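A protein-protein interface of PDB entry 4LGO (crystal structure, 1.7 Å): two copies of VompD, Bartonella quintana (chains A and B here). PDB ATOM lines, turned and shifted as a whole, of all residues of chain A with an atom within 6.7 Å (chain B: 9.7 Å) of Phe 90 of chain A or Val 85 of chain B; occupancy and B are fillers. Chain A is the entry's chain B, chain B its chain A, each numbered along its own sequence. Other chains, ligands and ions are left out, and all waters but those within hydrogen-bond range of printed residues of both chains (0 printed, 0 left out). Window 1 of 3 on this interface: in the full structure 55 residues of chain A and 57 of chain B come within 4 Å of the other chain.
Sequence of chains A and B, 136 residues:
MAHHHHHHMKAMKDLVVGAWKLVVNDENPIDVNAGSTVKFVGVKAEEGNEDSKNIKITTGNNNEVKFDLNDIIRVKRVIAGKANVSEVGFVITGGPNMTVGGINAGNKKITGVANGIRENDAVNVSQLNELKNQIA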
ATOM      1  N   VAL A  78      12.935 -21.745 -23.397  1.00  0.00           N
ATOM      2  CA  VAL A  78      11.594 -21.386 -23.003  1.00  0.00           C
ATOM      3  C   VAL A  78      11.493 -19.861 -23.084  1.00  0.00           C
ATOM      4  O   VAL A  78      12.334 -19.148 -22.519  1.00  0.00           O
ATOM      5  CB  VAL A  78      11.252 -21.824 -21.547  1.00  0.00           C
ATOM      6  CG1 VAL A  78       9.828 -21.414 -21.244  1.00  0.00           C
ATOM      7  CG2 VAL A  78      11.418 -23.307 -21.349  1.00  0.00           C
ATOM      8  N   ASN A  84      13.475 -15.435 -20.607  1.00  0.00           N
ATOM      9  CA  ASN A  84      14.080 -16.512 -21.395  1.00  0.00           C
ATOM     10  C   ASN A  84      14.872 -17.455 -20.518  1.00  0.00           C
ATOM     11  O   ASN A  84      15.651 -17.031 -19.653  1.00  0.00           O
ATOM     12  CB  ASN A  84      15.045 -15.962 -22.463  1.00  0.00           C
ATOM     13  CG  ASN A  84      14.333 -15.296 -23.604  1.00  0.00           C
ATOM     14  OD1 ASN A  84      14.216 -15.868 -24.698  1.00  0.00           O
ATOM     15  ND2 ASN A  84      13.866 -14.075 -23.381  1.00  0.00           N
ATOM     16  N   VAL A  85      14.643 -18.744 -20.727  1.00  0.00           N
ATOM     17  CA  VAL A  85      15.464 -19.794 -20.136  1.00  0.00           C
ATOM     18  C   VAL A  85      16.149 -20.479 -21.305  1.00  0.00           C
ATOM     19  O   VAL A  85      15.468 -20.929 -22.244  1.00  0.00           O
ATOM     20  CB  VAL A  85      14.600 -20.832 -19.408  1.00  0.00           C
ATOM     21  CG1 VAL A  85      15.462 -21.942 -18.779  1.00  0.00           C
ATOM     22  CG2 VAL A  85      13.728 -20.167 -18.354  1.00  0.00           C
ATOM     23  N   SER A  86      17.471 -20.590 -21.262  1.00  0.00           N
ATOM     24  CA  SER A  86      18.185 -21.278 -22.311  1.00  0.00           C
ATOM     25  C   SER A  86      19.523 -21.737 -21.777  1.00  0.00           C
ATOM     26  O   SER A  86      19.865 -21.526 -20.622  1.00  0.00           O
ATOM     27  CB  SER A  86      18.376 -20.341 -23.535  1.00  0.00           C
ATOM     28  OG  SER A  86      19.334 -19.362 -23.243  1.00  0.00           O
ATOM     29  N   VAL A  88      22.321 -20.455 -22.016  1.00  0.00           N
ATOM     30  CA  VAL A  88      23.109 -19.376 -21.395  1.00  0.00           C
ATOM     31  C   VAL A  88      22.673 -19.048 -19.978  1.00  0.00           C
ATOM     32  O   VAL A  88      23.453 -18.484 -19.212  1.00  0.00           O
ATOM     33  CB  VAL A  88      23.109 -18.099 -22.288  1.00  0.00           C
ATOM     34  CG1 VAL A  88      21.793 -17.346 -22.223  1.00  0.00           C
ATOM     35  CG2 VAL A  88      24.267 -17.184 -21.925  1.00  0.00           C
ATOM     36  N   GLY A  89      21.417 -19.365 -19.641  1.00  0.00           N
ATOM     37  CA  GLY A  89      20.887 -19.104 -18.334  1.00  0.00           C
ATOM     38  C   GLY A  89      19.498 -18.500 -18.348  1.00  0.00           C
ATOM     39  O   GLY A  89      18.668 -18.812 -19.215  1.00  0.00           O
ATOM     40  N   PHE A  90      19.276 -17.624 -17.376  1.00  0.00           N
ATOM     41  CA  PHE A  90      17.976 -17.029 -17.090  1.00  0.00           C
ATOM     42  C   PHE A  90      18.087 -15.564 -17.418  1.00  0.00           C
ATOM     43  O   PHE A  90      18.775 -14.841 -16.728  1.00  0.00           O
ATOM     44  CB  PHE A  90      17.574 -17.256 -15.610  1.00  0.00           C
ATOM     45  CG  PHE A  90      17.493 -18.714 -15.256  1.00  0.00           C
ATOM     46  CD1 PHE A  90      16.358 -19.434 -15.536  1.00  0.00           C
ATOM     47  CD2 PHE A  90      18.617 -19.403 -14.790  1.00  0.00           C
ATOM     48  CE1 PHE A  90      16.304 -20.787 -15.276  1.00  0.00           C
ATOM     49  CE2 PHE A  90      18.548 -20.760 -14.516  1.00  0.00           C
ATOM     50  CZ  PHE A  90      17.416 -21.449 -14.793  1.00  0.00           C
ATOM     51  N   VAL A  91      17.407 -15.130 -18.481  1.00  0.00           N
ATOM     52  CA  VAL A  91      17.590 -13.772 -18.987  1.00  0.00           C
ATOM     53  C   VAL A  91      16.263 -13.028 -19.103  1.00  0.00           C
ATOM     54  O   VAL A  91      15.326 -13.533 -19.675  1.00  0.00           O
ATOM     55  CB  VAL A  91      18.324 -13.793 -20.348  1.00  0.00           C
ATOM     56  CG1 VAL A  91      18.410 -12.404 -20.938  1.00  0.00           C
ATOM     57  CG2 VAL A  91      19.694 -14.427 -20.178  1.00  0.00           C
ATOM     58  N   ILE A  92      16.201 -11.824 -18.551  1.00  0.00           N
ATOM     59  CA  ILE A  92      15.075 -10.940 -18.807  1.00  0.00           C
ATOM     60  C   ILE A  92      15.564  -9.888 -19.788  1.00  0.00           C
ATOM     61  O   ILE A  92      16.483  -9.136 -19.472  1.00  0.00           O
ATOM     62  CB  ILE A  92      14.536 -10.278 -17.534  1.00  0.00           C
ATOM     63  CG1 ILE A  92      14.054 -11.357 -16.557  1.00  0.00           C
ATOM     64  CG2 ILE A  92      13.407  -9.305 -17.908  1.00  0.00           C
ATOM     65  CD1 ILE A  92      13.682 -10.851 -15.201  1.00  0.00           C
ATOM     66  N   PRO A  96      17.356  -7.824 -15.480  1.00  0.00           N
ATOM     67  CA  PRO A  96      18.333  -8.681 -14.810  1.00  0.00           C
ATOM     68  C   PRO A  96      18.594  -9.991 -15.539  1.00  0.00           C
ATOM     69  O   PRO A  96      17.785 -10.424 -16.390  1.00  0.00           O
ATOM     70  CB  PRO A  96      17.677  -8.988 -13.463  1.00  0.00           C
ATOM     71  CG  PRO A  96      16.694  -7.923 -13.244  1.00  0.00           C
ATOM     72  CD  PRO A  96      16.234  -7.483 -14.592  1.00  0.00           C
ATOM     73  N   ASN A  97      19.706 -10.628 -15.208  1.00  0.00           N
ATOM     74  CA  ASN A  97      19.968 -11.977 -15.700  1.00  0.00           C
ATOM     75  C   ASN A  97      20.874 -12.771 -14.757  1.00  0.00           C
ATOM     76  O   ASN A  97      21.525 -12.220 -13.870  1.00  0.00           O
ATOM     77  CB  ASN A  97      20.513 -11.947 -17.129  1.00  0.00           C
ATOM     78  CG  ASN A  97      21.898 -11.324 -17.210  1.00  0.00           C
ATOM     79  OD1 ASN A  97      22.842 -11.821 -16.605  1.00  0.00           O
ATOM     80  ND2 ASN A  97      22.015 -10.223 -17.916  1.00  0.00           N
ATOM     81  N   MET A  98      20.870 -14.090 -14.943  1.00  0.00           N
ATOM     82  CA  MET A  98      21.771 -15.000 -14.246  1.00  0.00           C
ATOM     83  C   MET A  98      22.337 -15.955 -15.285  1.00  0.00           C
ATOM     84  O   MET A  98      21.572 -16.722 -15.906  1.00  0.00           O
ATOM     85  CB  MET A  98      21.000 -15.758 -13.157  1.00  0.00           C
ATOM     86  CG  MET A  98      21.810 -16.682 -12.282  1.00  0.00           C
ATOM     87  SD  MET A  98      20.928 -17.282 -10.818  1.00  0.00           S
ATOM     88  CE  MET A  98      19.554 -18.204 -11.548  1.00  0.00           C
ATOM     89  N   THR A  99      23.654 -15.907 -15.468  1.00  0.00           N
ATOM     90  CA  THR A  99      24.358 -16.761 -16.443  1.00  0.00           C
ATOM     91  C   THR A  99      25.557 -17.425 -15.780  1.00  0.00           C
ATOM     92  O   THR A  99      25.805 -17.177 -14.609  1.00  0.00           O
ATOM     93  CB  THR A  99      24.846 -15.927 -17.654  1.00  0.00           C
ATOM     94  OG1 THR A  99      25.866 -15.023 -17.230  1.00  0.00           O
ATOM     95  CG2 THR A  99      23.694 -15.111 -18.245  1.00  0.00           C
ATOM     96  N   ILE B  73       1.857 -24.083 -18.351  1.00  0.00           N
ATOM     97  CA  ILE B  73       2.243 -25.477 -18.216  1.00  0.00           C
ATOM     98  C   ILE B  73       2.791 -25.751 -16.820  1.00  0.00           C
ATOM     99  O   ILE B  73       3.437 -24.891 -16.212  1.00  0.00           O
ATOM    100  CB  ILE B  73       3.234 -25.954 -19.311  1.00  0.00           C
ATOM    101  CG1 ILE B  73       4.557 -25.148 -19.325  1.00  0.00           C
ATOM    102  CG2 ILE B  73       2.547 -25.931 -20.679  1.00  0.00           C
ATOM    103  CD1 ILE B  73       5.635 -25.766 -20.197  1.00  0.00           C
ATOM    104  N   ARG B  74       2.480 -26.946 -16.330  1.00  0.00           N
ATOM    105  CA  ARG B  74       2.814 -27.400 -14.986  1.00  0.00           C
ATOM    106  C   ARG B  74       3.681 -28.650 -15.113  1.00  0.00           C
ATOM    107  O   ARG B  74       3.241 -29.706 -15.619  1.00  0.00           O
ATOM    108  CB  ARG B  74       1.508 -27.648 -14.169  1.00  0.00           C
ATOM    109  CG  ARG B  74       0.780 -26.382 -13.753  1.00  0.00           C
ATOM    110  CD  ARG B  74      -0.644 -26.693 -13.278  1.00  0.00           C
ATOM    111  NE  ARG B  74      -1.358 -25.491 -12.820  1.00  0.00           N
ATOM    112  CZ  ARG B  74      -2.088 -24.679 -13.590  1.00  0.00           C
ATOM    113  NH1 ARG B  74      -2.266 -24.920 -14.872  1.00  0.00           N
ATOM    114  NH2 ARG B  74      -2.697 -23.618 -13.034  1.00  0.00           N
ATOM    115  N   VAL B  75       4.925 -28.527 -14.662  1.00  0.00           N
ATOM    116  CA  VAL B  75       5.903 -29.604 -14.766  1.00  0.00           C
ATOM    117  C   VAL B  75       6.672 -29.684 -13.449  1.00  0.00           C
ATOM    118  O   VAL B  75       6.454 -28.886 -12.531  1.00  0.00           O
ATOM    119  CB  VAL B  75       6.893 -29.369 -15.960  1.00  0.00           C
ATOM    120  CG1 VAL B  75       6.128 -29.294 -17.293  1.00  0.00           C
ATOM    121  CG2 VAL B  75       7.739 -28.126 -15.744  1.00  0.00           C
ATOM    122  N   LYS B  76       7.591 -30.654 -13.335  1.00  0.00           N
ATOM    123  CA  LYS B  76       8.466 -30.646 -12.172  1.00  0.00           C
ATOM    124  C   LYS B  76       9.846 -30.121 -12.520  1.00  0.00           C
ATOM    125  O   LYS B  76      10.507 -29.558 -11.652  1.00  0.00           O
ATOM    126  CB  LYS B  76       8.562 -32.041 -11.600  1.00  0.00           C
ATOM    127  CG  LYS B  76       7.165 -32.570 -11.217  1.00  0.00           C
ATOM    128  CD  LYS B  76       7.068 -32.942  -9.814  1.00  0.00           C
ATOM    129  CE  LYS B  76       5.687 -33.495  -9.454  1.00  0.00           C
ATOM    130  NZ  LYS B  76       5.903 -34.618  -8.509  1.00  0.00           N
ATOM    131  N   ARG B  77      10.270 -30.300 -13.780  1.00  0.00           N
ATOM    132  CA  ARG B  77      11.613 -29.857 -14.181  1.00  0.00           C
ATOM    133  C   ARG B  77      11.623 -29.394 -15.630  1.00  0.00           C
ATOM    134  O   ARG B  77      10.993 -30.018 -16.475  1.00  0.00           O
ATOM    135  CB  ARG B  77      12.612 -31.001 -14.102  1.00  0.00           C
ATOM    136  CG  ARG B  77      12.815 -31.668 -12.748  1.00  0.00           C
ATOM    137  CD  ARG B  77      13.993 -31.067 -12.007  1.00  0.00           C
ATOM    138  NE  ARG B  77      15.263 -31.522 -12.570  1.00  0.00           N
ATOM    139  CZ  ARG B  77      16.037 -30.825 -13.400  1.00  0.00           C
ATOM    140  NH1 ARG B  77      15.729 -29.585 -13.792  1.00  0.00           N
ATOM    141  NH2 ARG B  77      17.165 -31.364 -13.833  1.00  0.00           N
ATOM    142  N   VAL B  78      12.323 -28.303 -15.888  1.00  0.00           N
ATOM    143  CA  VAL B  78      12.713 -27.926 -17.261  1.00  0.00           C
ATOM    144  C   VAL B  78      14.230 -27.961 -17.343  1.00  0.00           C
ATOM    145  O   VAL B  78      14.900 -27.386 -16.498  1.00  0.00           O
ATOM    146  CB  VAL B  78      12.209 -26.510 -17.688  1.00  0.00           C
ATOM    147  CG1 VAL B  78      12.653 -26.241 -19.146  1.00  0.00           C
ATOM    148  CG2 VAL B  78      10.711 -26.386 -17.481  1.00  0.00           C
ATOM    149  N   ILE B  79      14.782 -28.661 -18.341  1.00  0.00           N
ATOM    150  CA  ILE B  79      16.215 -28.725 -18.557  1.00  0.00           C
ATOM    151  C   ILE B  79      16.513 -28.067 -19.903  1.00  0.00           C
ATOM    152  O   ILE B  79      16.011 -28.495 -20.920  1.00  0.00           O
ATOM    153  CB  ILE B  79      16.745 -30.179 -18.573  1.00  0.00           C
ATOM    154  CG1 ILE B  79      16.358 -30.932 -17.294  1.00  0.00           C
ATOM    155  CG2 ILE B  79      18.260 -30.194 -18.774  1.00  0.00           C
ATOM    156  CD1 ILE B  79      16.682 -32.408 -17.327  1.00  0.00           C
ATOM    157  N   ALA B  80      17.292 -26.998 -19.881  1.00  0.00           N
ATOM    158  CA  ALA B  80      17.722 -26.334 -21.117  1.00  0.00           C
ATOM    159  C   ALA B  80      19.211 -26.159 -21.039  1.00  0.00           C
ATOM    160  O   ALA B  80      19.707 -25.134 -20.534  1.00  0.00           O
ATOM    161  CB  ALA B  80      17.003 -24.997 -21.264  1.00  0.00           C
ATOM    162  N   GLY B  81      19.943 -27.182 -21.500  1.00  0.00           N
ATOM    163  CA  GLY B  81      21.378 -27.223 -21.300  1.00  0.00           C
ATOM    164  C   GLY B  81      21.723 -27.227 -19.820  1.00  0.00           C
ATOM    165  O   GLY B  81      21.150 -27.996 -19.056  1.00  0.00           O
ATOM    166  N   LYS B  82      22.603 -26.321 -19.407  1.00  0.00           N
ATOM    167  CA  LYS B  82      22.988 -26.248 -17.995  1.00  0.00           C
ATOM    168  C   LYS B  82      21.996 -25.454 -17.154  1.00  0.00           C
ATOM    169  O   LYS B  82      22.178 -25.363 -15.957  1.00  0.00           O
ATOM    170  CB  LYS B  82      24.402 -25.683 -17.809  1.00  0.00           C
ATOM    171  CG  LYS B  82      24.646 -24.299 -18.362  1.00  0.00           C
ATOM    172  CD  LYS B  82      26.151 -24.059 -18.470  1.00  0.00           C
ATOM    173  CE  LYS B  82      26.459 -22.629 -18.899  1.00  0.00           C
ATOM    174  NZ  LYS B  82      26.403 -22.475 -20.384  1.00  0.00           N
ATOM    175  N   ALA B  83      20.995 -24.837 -17.777  1.00  0.00           N
ATOM    176  CA  ALA B  83      19.942 -24.121 -17.034  1.00  0.00           C
ATOM    177  C   ALA B  83      18.789 -25.052 -16.648  1.00  0.00           C
ATOM    178  O   ALA B  83      18.230 -25.766 -17.481  1.00  0.00           O
ATOM    179  CB  ALA B  83      19.406 -22.968 -17.843  1.00  0.00           C
ATOM    180  N   ASN B  84      18.451 -25.053 -15.364  1.00  0.00           N
ATOM    181  CA  ASN B  84      17.424 -25.947 -14.822  1.00  0.00           C
ATOM    182  C   ASN B  84      16.382 -25.217 -14.003  1.00  0.00           C
ATOM    183  O   ASN B  84      16.707 -24.420 -13.112  1.00  0.00           O
ATOM    184  CB  ASN B  84      18.079 -26.996 -13.906  1.00  0.00           C
ATOM    185  CG  ASN B  84      18.842 -28.008 -14.680  1.00  0.00           C
ATOM    186  OD1 ASN B  84      18.296 -29.054 -15.035  1.00  0.00           O
ATOM    187  ND2 ASN B  84      20.088 -27.694 -15.024  1.00  0.00           N
ATOM    188  N   VAL B  85      15.127 -25.480 -14.310  1.00  0.00           N
ATOM    189  CA  VAL B  85      14.008 -25.044 -13.477  1.00  0.00           C
ATOM    190  C   VAL B  85      13.465 -26.258 -12.727  1.00  0.00           C
ATOM    191  O   VAL B  85      13.259 -27.321 -13.311  1.00  0.00           O
ATOM    192  CB  VAL B  85      12.888 -24.421 -14.325  1.00  0.00           C
ATOM    193  CG1 VAL B  85      11.735 -24.003 -13.433  1.00  0.00           C
ATOM    194  CG2 VAL B  85      13.370 -23.214 -15.106  1.00  0.00           C
ATOM    195  N   SER B  86      13.181 -26.098 -11.436  1.00  0.00           N
ATOM    196  CA  SER B  86      12.652 -27.208 -10.642  1.00  0.00           C
ATOM    197  C   SER B  86      11.873 -26.634  -9.494  1.00  0.00           C
ATOM    198  O   SER B  86      11.848 -25.422  -9.340  1.00  0.00           O
ATOM    199  CB  SER B  86      13.784 -28.056 -10.093  1.00  0.00           C
ATOM    200  OG  SER B  86      14.430 -27.445  -9.014  1.00  0.00           O
ATOM    201  N   GLU B  87      11.289 -27.510  -8.665  1.00  0.00           N
ATOM    202  CA  GLU B  87      10.545 -27.093  -7.497  1.00  0.00           C
ATOM    203  C   GLU B  87      11.384 -26.310  -6.509  1.00  0.00           C
ATOM    204  O   GLU B  87      10.821 -25.692  -5.639  1.00  0.00           O
ATOM    205  CB  GLU B  87       9.910 -28.329  -6.807  1.00  0.00           C
ATOM    206  CG  GLU B  87       8.827 -28.951  -7.706  1.00  0.00           C
ATOM    207  CD  GLU B  87       8.455 -30.410  -7.378  1.00  0.00           C
ATOM    208  OE1 GLU B  87       9.353 -31.273  -7.271  1.00  0.00           O
ATOM    209  OE2 GLU B  87       7.246 -30.700  -7.317  1.00  0.00           O
ATOM    210  N   VAL B  88      12.717 -26.414  -6.607  1.00  0.00           N
ATOM    211  CA  VAL B  88      13.650 -25.657  -5.741  1.00  0.00           C
ATOM    212  C   VAL B  88      14.007 -24.281  -6.313  1.00  0.00           C
ATOM    213  O   VAL B  88      14.515 -23.437  -5.575  1.00  0.00           O
ATOM    214  CB  VAL B  88      14.931 -26.455  -5.325  1.00  0.00           C
ATOM    215  CG1 VAL B  88      14.579 -27.847  -4.825  1.00  0.00           C
ATOM    216  CG2 VAL B  88      15.944 -26.566  -6.434  1.00  0.00           C
ATOM    217  N   GLY B  89      13.705 -24.034  -7.599  1.00  0.00           N
ATOM    218  CA  GLY B  89      14.003 -22.748  -8.186  1.00  0.00           C
ATOM    219  C   GLY B  89      14.816 -22.877  -9.465  1.00  0.00           C
ATOM    220  O   GLY B  89      14.559 -23.743 -10.302  1.00  0.00           O
ATOM    221  N   PHE B  90      15.786 -21.986  -9.611  1.00  0.00           N
ATOM    222  CA  PHE B  90      16.490 -21.733 -10.852  1.00  0.00           C
ATOM    223  C   PHE B  90      17.984 -21.959 -10.657  1.00  0.00           C
ATOM    224  O   PHE B  90      18.618 -21.268  -9.855  1.00  0.00           O
ATOM    225  CB  PHE B  90      16.198 -20.280 -11.281  1.00  0.00           C
ATOM    226  CG  PHE B  90      14.724 -19.970 -11.313  1.00  0.00           C
ATOM    227  CD1 PHE B  90      13.928 -20.384 -12.392  1.00  0.00           C
ATOM    228  CD2 PHE B  90      14.105 -19.351 -10.238  1.00  0.00           C
ATOM    229  CE1 PHE B  90      12.577 -20.148 -12.370  1.00  0.00           C
ATOM    230  CE2 PHE B  90      12.747 -19.101 -10.219  1.00  0.00           C
ATOM    231  CZ  PHE B  90      11.978 -19.502 -11.296  1.00  0.00           C
ATOM    232  N   VAL B  91      18.542 -22.908 -11.402  1.00  0.00           N
ATOM    233  CA  VAL B  91      19.931 -23.366 -11.178  1.00  0.00           C
ATOM    234  C   VAL B  91      20.695 -23.375 -12.496  1.00  0.00           C
ATOM    235  O   VAL B  91      20.218 -23.909 -13.520  1.00  0.00           O
ATOM    236  CB  VAL B  91      19.935 -24.795 -10.585  1.00  0.00           C
ATOM    237  CG1 VAL B  91      21.330 -25.354 -10.476  1.00  0.00           C
ATOM    238  CG2 VAL B  91      19.201 -24.809  -9.239  1.00  0.00           C
ATOM    239  N   ILE B  92      21.886 -22.795 -12.475  1.00  0.00           N
ATOM    240  CA  ILE B  92      22.841 -23.037 -13.543  1.00  0.00           C
ATOM    241  C   ILE B  92      23.826 -24.073 -13.028  1.00  0.00           C
ATOM    242  O   ILE B  92      24.500 -23.833 -12.015  1.00  0.00           O
ATOM    243  CB  ILE B  92      23.605 -21.759 -13.898  1.00  0.00           C
ATOM    244  CG1 ILE B  92      22.633 -20.588 -14.104  1.00  0.00           C
ATOM    245  CG2 ILE B  92      24.491 -21.993 -15.112  1.00  0.00           C
ATOM    246  CD1 ILE B  92      22.227 -20.290 -15.495  1.00  0.00           C
ATOM    247  N   THR B  93      23.918 -25.198 -13.725  1.00  0.00           N
ATOM    248  CA  THR B  93      24.909 -26.222 -13.392  1.00  0.00           C
ATOM    249  C   THR B  93      26.316 -25.667 -13.436  1.00  0.00           C
ATOM    250  O   THR B  93      26.737 -25.061 -14.414  1.00  0.00           O
ATOM    251  CB  THR B  93      24.784 -27.419 -14.334  1.00  0.00           C
ATOM    252  OG1 THR B  93      23.438 -27.860 -14.262  1.00  0.00           O
ATOM    253  CG2 THR B  93      25.752 -28.527 -13.930  1.00  0.00           C
ATOM    254  N   GLY B  95      27.257 -23.089 -11.762  1.00  0.00           N
ATOM    255  CA  GLY B  95      27.160 -21.643 -11.771  1.00  0.00           C
ATOM    256  C   GLY B  95      26.313 -21.125 -10.623  1.00  0.00           C
ATOM    257  O   GLY B  95      26.102 -21.841  -9.628  1.00  0.00           O
ATOM    258  N   PRO B  96      25.788 -19.901 -10.764  1.00  0.00           N
ATOM    259  CA  PRO B  96      24.920 -19.329  -9.733  1.00  0.00           C
ATOM    260  C   PRO B  96      23.563 -20.032  -9.657  1.00  0.00           C
ATOM    261  O   PRO B  96      23.183 -20.790 -10.571  1.00  0.00           O
ATOM    262  CB  PRO B  96      24.716 -17.880 -10.186  1.00  0.00           C
ATOM    263  CG  PRO B  96      25.588 -17.699 -11.386  1.00  0.00           C
ATOM    264  CD  PRO B  96      25.910 -19.014 -11.930  1.00  0.00           C
ATOM    265  N   ASN B  97      22.849 -19.794  -8.562  1.00  0.00           N
ATOM    266  CA  ASN B  97      21.477 -20.244  -8.454  1.00  0.00           C
ATOM    267  C   ASN B  97      20.602 -19.264  -7.696  1.00  0.00           C
ATOM    268  O   ASN B  97      21.104 -18.413  -6.982  1.00  0.00           O
ATOM    269  CB  ASN B  97      21.408 -21.667  -7.878  1.00  0.00           C
ATOM    270  CG  ASN B  97      21.774 -21.743  -6.422  1.00  0.00           C
ATOM    271  OD1 ASN B  97      21.129 -21.133  -5.571  1.00  0.00           O
ATOM    272  ND2 ASN B  97      22.795 -22.556  -6.107  1.00  0.00           N
ATOM    273  N   MET B  98      19.296 -19.378  -7.917  1.00  0.00           N
ATOM    274  CA  MET B  98      18.311 -18.644  -7.160  1.00  0.00           C
ATOM    275  C   MET B  98      17.281 -19.682  -6.763  1.00  0.00           C
ATOM    276  O   MET B  98      16.466 -20.084  -7.588  1.00  0.00           O
ATOM    277  CB  MET B  98      17.662 -17.526  -7.995  1.00  0.00           C
ATOM    278  CG  MET B  98      16.602 -16.807  -7.184  1.00  0.00           C
ATOM    279  SD  MET B  98      15.873 -15.420  -8.076  1.00  0.00           S
ATOM    280  CE  MET B  98      14.959 -16.303  -9.289  1.00  0.00           C
ATOM    281  N   THR B  99      17.373 -20.163  -5.525  1.00  0.00           N
ATOM    282  CA  THR B  99      16.513 -21.262  -5.053  1.00  0.00           C
ATOM    283  C   THR B  99      15.849 -20.873  -3.738  1.00  0.00           C
ATOM    284  O   THR B  99      16.074 -19.779  -3.186  1.00  0.00           O
ATOM    285  CB  THR B  99      17.344 -22.536  -4.867  1.00  0.00           C
ATOM    286  OG1 THR B  99      18.385 -22.264  -3.941  1.00  0.00           O
ATOM    287  CG2 THR B  99      17.938 -22.987  -6.188  1.00  0.00           C
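The guanidinium group (NH1) of Arg 77 of chain B sits close to the backbone carbonyl oxygen (O) of Val 85 of chain B (3.4 Å). O of Phe 90 of chain A lies within hydrogen-bond range of N of Met 98 of chain A (2.9 Å). The backbone carbonyl oxygen of Val 78 of chain B sits at hydrogen-bond distance from the backbone NH of Val 85 of chain B (2.9 Å). The side-chain amide nitrogen of Asn 84 of chain B lies within hydrogen-bond range of the side-chain hydroxyl of Thr 93 of chain B (3.4 Å). The side-chain amide oxygen of Asn 97 of chain B sits at hydrogen-bond distance from the side-chain hydroxyl of Thr 99 of chain B, 3.4 Å away. The backbone NH of Val 88 of chain A lies close to the side-chain hydroxyl of Ser 86 of chain A.
Gly 89 of chain A touches Ile 92 of chain B, but with the chains exchanged Ile 92 of chain A does not touch Gly 89 of chain B (13.4 Å). Phe 90 of chain A touches Asn 84 of chain B, but with the chains exchanged Asn 84 of chain A does not touch Phe 90 of chain B (8.2 Å). Phe 90 of chain A touches its own counterpart, Phe 90 of chain B. Met 98 of chain A touches Asn 97 of chain B, but with the chains exchanged Asn 97 of chain A does not touch Met 98 of chain B (8.7 Å). Positions printed for both chains: 78, 84, 85, 86, 88, 89, 90, 91, 92, 96, 97, 98 and 99. Of the 16 pairs that touch across the chains among the printed residues, 3 have their exchanged pair printed and touching as well.
Val 85 of chain A touches none of the printed residues of chain B. Gly 89 of chain A touches just one residue of chain B: Ile 92. Of chain B, only Ala 83, Asn 84, Val 85, Phe 90, Val 91 and Ile 92 come within 4 Å of Phe 90 of chain A. No residue of chain B comes within 4 Å of Val 91 of chain A. Of the printed residues of chain B, Thr 99 of chain A touches Pro 96 (3.3 Å). Printed residues of chain A within 4 Å of Ala 80 of chain B: Ser 86 (3.6 Å). Printed residues of chain A within 4 Å of Ala 83 of chain B: Ser 86 (3.2 Å) and Phe 90 (3.9 Å). Of chain A, only Phe 90 (3.8 Å) comes within 4 Å of Val 85 of chain B. Of the printed residues of chain A, Phe 90 of chain B touches Phe 90 and Met 98. The nearest printed residue of chain A that does not touch Ile 92 of chain B is Thr 99 of chain A (4.2 Å).
Ser 86 of chain A touches Ala 80 of chain B. O of Ser 86 of chain A touches CB of Ala 83 of chain B, 3.2 Å away. CZ of Phe 90 of chain A touches CB of Ala 83 of chain B, 3.9 Å away. CZ of Phe 90 of chain A touches O of Asn 84 of chain B, 3.5 Å away. Val 85 of chain B touches Phe 90 of chain A (CG2 to CE1, 3.8 Å). Phe 90 of chain A touches Phe 90 of chain B (CE1 to CD1, 3.8 Å). Phe 90 of chain A touches Val 91 of chain B (CE2 to O, 3.7 Å). CD2 of Phe 90 of chain A touches CD1 of Ile 92 of chain B, 3.8 Å away. Met 98 of chain A touches Pro 96 of chain B (CG to CB, 3.8 Å). Met 98 of chain A touches Asn 97 of chain B.
Printed residues of chain B that touch a printed residue of chain A: Val 78, Ala 80, Ala 83, Asn 84, Val 85, Phe 90, Val 91, Ile 92, Pro 96, Asn 97 and Met 98. Hydrophobic or aromatic side chains of chain B within 4 Å of the printed part of chain A: Val 78, Ala 83, Val 85, Phe 90, Ile 92 and Pro 96. Of the 13 printed residues of chain A, 6 touch a printed residue of chain B. Hydrophobic or aromatic side chains of chain A within 4 Å of the printed part of chain B: Val 78, Phe 90 and Met 98. Among the printed residues, 16 pairs touch across the chains.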
